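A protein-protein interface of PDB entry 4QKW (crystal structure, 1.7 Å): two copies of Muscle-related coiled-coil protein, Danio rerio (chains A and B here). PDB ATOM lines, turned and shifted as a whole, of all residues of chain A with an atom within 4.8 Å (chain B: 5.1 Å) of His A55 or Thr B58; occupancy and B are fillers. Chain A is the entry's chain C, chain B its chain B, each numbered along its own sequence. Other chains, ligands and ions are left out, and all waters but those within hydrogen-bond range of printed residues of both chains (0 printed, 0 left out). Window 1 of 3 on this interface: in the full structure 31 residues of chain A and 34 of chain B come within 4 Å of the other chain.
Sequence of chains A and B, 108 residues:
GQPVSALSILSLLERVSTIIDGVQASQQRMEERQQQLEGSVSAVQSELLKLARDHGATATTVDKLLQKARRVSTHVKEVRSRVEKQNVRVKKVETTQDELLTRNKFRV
O of Asp B54 is in hydrogen-bond range of OG1 of Thr B58 (3.3 Å).
The backbone carbonyl oxygen (O) of Ala B57 is in hydrogen-bond range of the side-chain hydroxyl (OG1) of Thr B61 (3.2 Å).
Printed residues of chain B within 4 Å of His A55: Asp B54, His B55 and Thr B58.
Of chain A, only His A55 (2.7 Å) comes within 4 Å of Thr B58.
Of the printed residues of chain A, Leu B51 touches Leu A51 and Ala A52.
Of the printed residues of chain B, Ala A52 touches Leu B51.
Printed residues of chain A within 4 Å of Asp B54: His A55.
Printed residues of chain B within 4 Å of Leu A51: Leu B51 (3.9 Å).
Of the printed residues of chain A, Thr B61 touches Val A62 (3.6 Å).
The nearest residue of chain B that does not touch His A55 is Leu B51 (4.04 Å).
Hydrophobic or aromatic side chains of chain B that line the printed part of chain A: Leu B51, His B55 and Val B62.
Hydrophobic or aromatic side chains of chain A within 4 Å of the printed part of chain B: Leu A51, His A55 and Val A62.
OG1 of Thr B58 is in hydrogen-bond range of NE2 of His A55, at 2.7 Å.
Among the printed residues, pairs that only touch across the chains: His A55 with His B55, Val A62 with Thr B61, His A55 with Asp B54, Ala A52 with Leu B51, Val A62 with Val B62 and Leu A51 with Leu B51.
Leu A51 touches its own counterpart, Leu B51.
His A55 touches Asp B54, but with the chains exchanged Asp A54 does not touch His B55 (8.3 Å).
His B55 touches its own counterpart, His A55.
Val B62 touches its own counterpart, Val A62.
Positions printed for both chains: 51, 54, 55, 56, 57, 58, 59 and 62.
Of the 7 pairs that touch across the chains among the printed residues, 3 have their exchanged pair printed and touching as well.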
ATOM      1  N   LEU A  51      -7.209  -7.109  20.075  1.00  0.00           N
ATOM      2  CA  LEU A  51      -6.262  -6.750  21.134  1.00  0.00           C
ATOM      3  C   LEU A  51      -5.525  -5.470  20.770  1.00  0.00           C
ATOM      4  O   LEU A  51      -5.274  -4.608  21.631  1.00  0.00           O
ATOM      5  CB  LEU A  51      -5.258  -7.893  21.361  1.00  0.00           C
ATOM      6  CG  LEU A  51      -4.283  -7.683  22.521  1.00  0.00           C
ATOM      7  CD1 LEU A  51      -5.047  -7.324  23.769  1.00  0.00           C
ATOM      8  CD2 LEU A  51      -3.448  -8.924  22.774  1.00  0.00           C
ATOM      9  N   ALA A  52      -5.199  -5.333  19.488  1.00  0.00           N
ATOM     10  CA  ALA A  52      -4.517  -4.146  18.990  1.00  0.00           C
ATOM     11  C   ALA A  52      -5.377  -2.913  19.225  1.00  0.00           C
ATOM     12  O   ALA A  52      -4.878  -1.865  19.647  1.00  0.00           O
ATOM     13  CB  ALA A  52      -4.183  -4.298  17.507  1.00  0.00           C
ATOM     14  N   ARG A  53      -6.674  -3.046  18.960  1.00  0.00           N
ATOM     15  CA  ARG A  53      -7.609  -1.944  19.188  1.00  0.00           C
ATOM     16  C   ARG A  53      -7.701  -1.630  20.668  1.00  0.00           C
ATOM     17  O   ARG A  53      -7.738  -0.450  21.061  1.00  0.00           O
ATOM     18  CB  ARG A  53      -9.009  -2.304  18.676  1.00  0.00           C
ATOM     19  CG  ARG A  53      -9.099  -2.542  17.182  1.00  0.00           C
ATOM     20  CD  ARG A  53     -10.550  -2.521  16.698  1.00  0.00           C
ATOM     21  NE  ARG A  53     -11.363  -3.617  17.232  1.00  0.00           N
ATOM     22  CZ  ARG A  53     -11.634  -4.742  16.573  1.00  0.00           C
ATOM     23  NH1 ARG A  53     -11.152  -4.927  15.350  1.00  0.00           N
ATOM     24  NH2 ARG A  53     -12.392  -5.682  17.130  1.00  0.00           N
ATOM     25  N   ASP A  54      -7.779  -2.676  21.491  1.00  0.00           N
ATOM     26  CA  ASP A  54      -7.860  -2.503  22.939  1.00  0.00           C
ATOM     27  C   ASP A  54      -6.627  -1.780  23.450  1.00  0.00           C
ATOM     28  O   ASP A  54      -6.734  -0.815  24.210  1.00  0.00           O
ATOM     29  CB  ASP A  54      -7.998  -3.846  23.657  1.00  0.00           C
ATOM     30  CG  ASP A  54      -9.341  -4.511  23.418  1.00  0.00           C
ATOM     31  OD1 ASP A  54     -10.271  -3.836  22.937  1.00  0.00           O
ATOM     32  OD2 ASP A  54      -9.456  -5.721  23.720  1.00  0.00           O
ATOM     33  N   HIS A  55      -5.451  -2.228  23.032  1.00  0.00           N
ATOM     34  CA  HIS A  55      -4.233  -1.534  23.449  1.00  0.00           C
ATOM     35  C   HIS A  55      -4.223  -0.081  22.987  1.00  0.00           C
ATOM     36  O   HIS A  55      -3.806   0.811  23.738  1.00  0.00           O
ATOM     37  CB  HIS A  55      -2.971  -2.229  22.954  1.00  0.00           C
ATOM     38  CG  HIS A  55      -1.730  -1.436  23.220  1.00  0.00           C
ATOM     39  ND1 HIS A  55      -1.121  -0.664  22.255  1.00  0.00           N
ATOM     40  CD2 HIS A  55      -1.016  -1.254  24.357  1.00  0.00           C
ATOM     41  CE1 HIS A  55      -0.072  -0.053  22.780  1.00  0.00           C
ATOM     42  NE2 HIS A  55       0.012  -0.391  24.055  1.00  0.00           N
ATOM     43  N   GLY A  56      -4.672   0.168  21.755  1.00  0.00           N
ATOM     44  CA  GLY A  56      -4.703   1.538  21.239  1.00  0.00           C
ATOM     45  C   GLY A  56      -5.550   2.457  22.098  1.00  0.00           C
ATOM     46  O   GLY A  56      -5.216   3.629  22.315  1.00  0.00           O
ATOM     47  N   ALA A  57      -6.657   1.925  22.604  1.00  0.00           N
ATOM     48  CA  ALA A  57      -7.518   2.688  23.501  1.00  0.00           C
ATOM     49  C   ALA A  57      -6.793   3.009  24.813  1.00  0.00           C
ATOM     50  O   ALA A  57      -6.885   4.127  25.338  1.00  0.00           O
ATOM     51  CB  ALA A  57      -8.805   1.920  23.766  1.00  0.00           C
ATOM     52  N   THR A  58      -6.088   2.018  25.347  1.00  0.00           N
ATOM     53  CA  THR A  58      -5.306   2.189  26.565  1.00  0.00           C
ATOM     54  C   THR A  58      -4.197   3.218  26.372  1.00  0.00           C
ATOM     55  O   THR A  58      -3.970   4.085  27.235  1.00  0.00           O
ATOM     56  CB  THR A  58      -4.679   0.859  27.000  1.00  0.00           C
ATOM     57  OG1 THR A  58      -5.719  -0.078  27.307  1.00  0.00           O
ATOM     58  CG2 THR A  58      -3.785   1.056  28.222  1.00  0.00           C
ATOM     59  N   ALA A  59      -3.506   3.134  25.237  1.00  0.00           N
ATOM     60  CA  ALA A  59      -2.424   4.074  24.950  1.00  0.00           C
ATOM     61  C   ALA A  59      -2.985   5.486  24.822  1.00  0.00           C
ATOM     62  O   ALA A  59      -2.367   6.454  25.278  1.00  0.00           O
ATOM     63  CB  ALA A  59      -1.682   3.665  23.687  1.00  0.00           C
ATOM     64  N   VAL A  62      -3.590   6.686  28.294  1.00  0.00           N
ATOM     65  CA  VAL A  62      -2.303   6.963  28.921  1.00  0.00           C
ATOM     66  C   VAL A  62      -1.756   8.341  28.530  1.00  0.00           C
ATOM     67  O   VAL A  62      -1.268   9.077  29.388  1.00  0.00           O
ATOM     68  CB  VAL A  62      -1.273   5.870  28.610  1.00  0.00           C
ATOM     69  CG1 VAL A  62       0.130   6.387  28.882  1.00  0.00           C
ATOM     70  CG2 VAL A  62      -1.571   4.643  29.449  1.00  0.00           C
ATOM     71  N   LEU B  51       2.984  -5.730  18.486  1.00  0.00           N
ATOM     72  CA  LEU B  51       2.035  -5.292  19.502  1.00  0.00           C
ATOM     73  C   LEU B  51       2.599  -5.473  20.920  1.00  0.00           C
ATOM     74  O   LEU B  51       2.403  -4.620  21.798  1.00  0.00           O
ATOM     75  CB  LEU B  51       0.696  -6.014  19.329  1.00  0.00           C
ATOM     76  CG  LEU B  51      -0.418  -5.554  20.262  1.00  0.00           C
ATOM     77  CD1 LEU B  51      -0.673  -4.050  20.099  1.00  0.00           C
ATOM     78  CD2 LEU B  51      -1.686  -6.359  19.990  1.00  0.00           C
ATOM     79  N   ASP B  54       5.009  -2.666  21.518  1.00  0.00           N
ATOM     80  CA  ASP B  54       4.238  -1.437  21.746  1.00  0.00           C
ATOM     81  C   ASP B  54       3.641  -1.397  23.155  1.00  0.00           C
ATOM     82  O   ASP B  54       3.655  -0.353  23.834  1.00  0.00           O
ATOM     83  CB  ASP B  54       3.128  -1.297  20.696  1.00  0.00           C
ATOM     84  CG  ASP B  54       3.648  -0.827  19.350  1.00  0.00           C
ATOM     85  OD1 ASP B  54       4.794  -0.332  19.295  1.00  0.00           O
ATOM     86  OD2 ASP B  54       2.906  -0.945  18.348  1.00  0.00           O
ATOM     87  N   HIS B  55       3.128  -2.539  23.609  1.00  0.00           N
ATOM     88  CA  HIS B  55       2.582  -2.622  24.958  1.00  0.00           C
ATOM     89  C   HIS B  55       3.680  -2.461  26.012  1.00  0.00           C
ATOM     90  O   HIS B  55       3.460  -1.864  27.071  1.00  0.00           O
ATOM     91  CB  HIS B  55       1.829  -3.938  25.178  1.00  0.00           C
ATOM     92  CG  HIS B  55       1.461  -4.158  26.609  1.00  0.00           C
ATOM     93  ND1 HIS B  55       2.170  -5.002  27.432  1.00  0.00           N
ATOM     94  CD2 HIS B  55       0.505  -3.586  27.382  1.00  0.00           C
ATOM     95  CE1 HIS B  55       1.649  -4.967  28.648  1.00  0.00           C
ATOM     96  NE2 HIS B  55       0.639  -4.116  28.643  1.00  0.00           N
ATOM     97  N   GLY B  56       4.877  -2.961  25.713  1.00  0.00           N
ATOM     98  CA  GLY B  56       5.997  -2.823  26.630  1.00  0.00           C
ATOM     99  C   GLY B  56       6.261  -1.357  26.905  1.00  0.00           C
ATOM    100  O   GLY B  56       6.503  -0.960  28.053  1.00  0.00           O
ATOM    101  N   ALA B  57       6.190  -0.544  25.856  1.00  0.00           N
ATOM    102  CA  ALA B  57       6.404   0.899  26.008  1.00  0.00           C
ATOM    103  C   ALA B  57       5.271   1.529  26.805  1.00  0.00           C
ATOM    104  O   ALA B  57       5.503   2.390  27.663  1.00  0.00           O
ATOM    105  CB  ALA B  57       6.550   1.573  24.645  1.00  0.00           C
ATOM    106  N   THR B  58       4.038   1.116  26.528  1.00  0.00           N
ATOM    107  CA  THR B  58       2.910   1.637  27.304  1.00  0.00           C
ATOM    108  C   THR B  58       3.024   1.301  28.790  1.00  0.00           C
ATOM    109  O   THR B  58       2.791   2.152  29.661  1.00  0.00           O
ATOM    110  CB  THR B  58       1.587   1.104  26.776  1.00  0.00           C
ATOM    111  OG1 THR B  58       1.431   1.518  25.416  1.00  0.00           O
ATOM    112  CG2 THR B  58       0.418   1.644  27.627  1.00  0.00           C
ATOM    113  N   ALA B  59       3.395   0.062  29.080  1.00  0.00           N
ATOM    114  CA  ALA B  59       3.542  -0.402  30.452  1.00  0.00           C
ATOM    115  C   ALA B  59       4.621   0.378  31.217  1.00  0.00           C
ATOM    116  O   ALA B  59       4.487   0.633  32.420  1.00  0.00           O
ATOM    117  CB  ALA B  59       3.853  -1.915  30.452  1.00  0.00           C
ATOM    118  N   THR B  60       5.692   0.755  30.518  1.00  0.00           N
ATOM    119  CA  THR B  60       6.754   1.560  31.117  1.00  0.00           C
ATOM    120  C   THR B  60       6.242   2.951  31.477  1.00  0.00           C
ATOM    121  O   THR B  60       6.505   3.459  32.567  1.00  0.00           O
ATOM    122  CB  THR B  60       7.960   1.701  30.173  1.00  0.00           C
ATOM    123  OG1 THR B  60       8.524   0.408  29.934  1.00  0.00           O
ATOM    124  CG2 THR B  60       9.020   2.602  30.785  1.00  0.00           C
ATOM    125  N   THR B  61       5.506   3.561  30.556  1.00  0.00           N
ATOM    126  CA  THR B  61       4.936   4.891  30.798  1.00  0.00           C
ATOM    127  C   THR B  61       3.985   4.849  31.986  1.00  0.00           C
ATOM    128  O   THR B  61       3.946   5.788  32.804  1.00  0.00           O
ATOM    129  CB  THR B  61       4.216   5.409  29.542  1.00  0.00           C
ATOM    130  OG1 THR B  61       5.160   5.478  28.463  1.00  0.00           O
ATOM    131  CG2 THR B  61       3.615   6.807  29.787  1.00  0.00           C
ATOM    132  N   VAL B  62       3.222   3.763  32.092  1.00  0.00           N
ATOM    133  CA  VAL B  62       2.285   3.608  33.205  1.00  0.00           C
ATOM    134  C   VAL B  62       3.033   3.522  34.532  1.00  0.00           C
ATOM    135  O   VAL B  62       2.619   4.126  35.525  1.00  0.00           O
ATOM    136  CB  VAL B  62       1.367   2.383  33.003  1.00  0.00           C
ATOM    137  CG1 VAL B  62       0.633   2.037  34.297  1.00  0.00           C
ATOM    138  CG2 VAL B  62       0.381   2.654  31.891  1.00  0.00           C
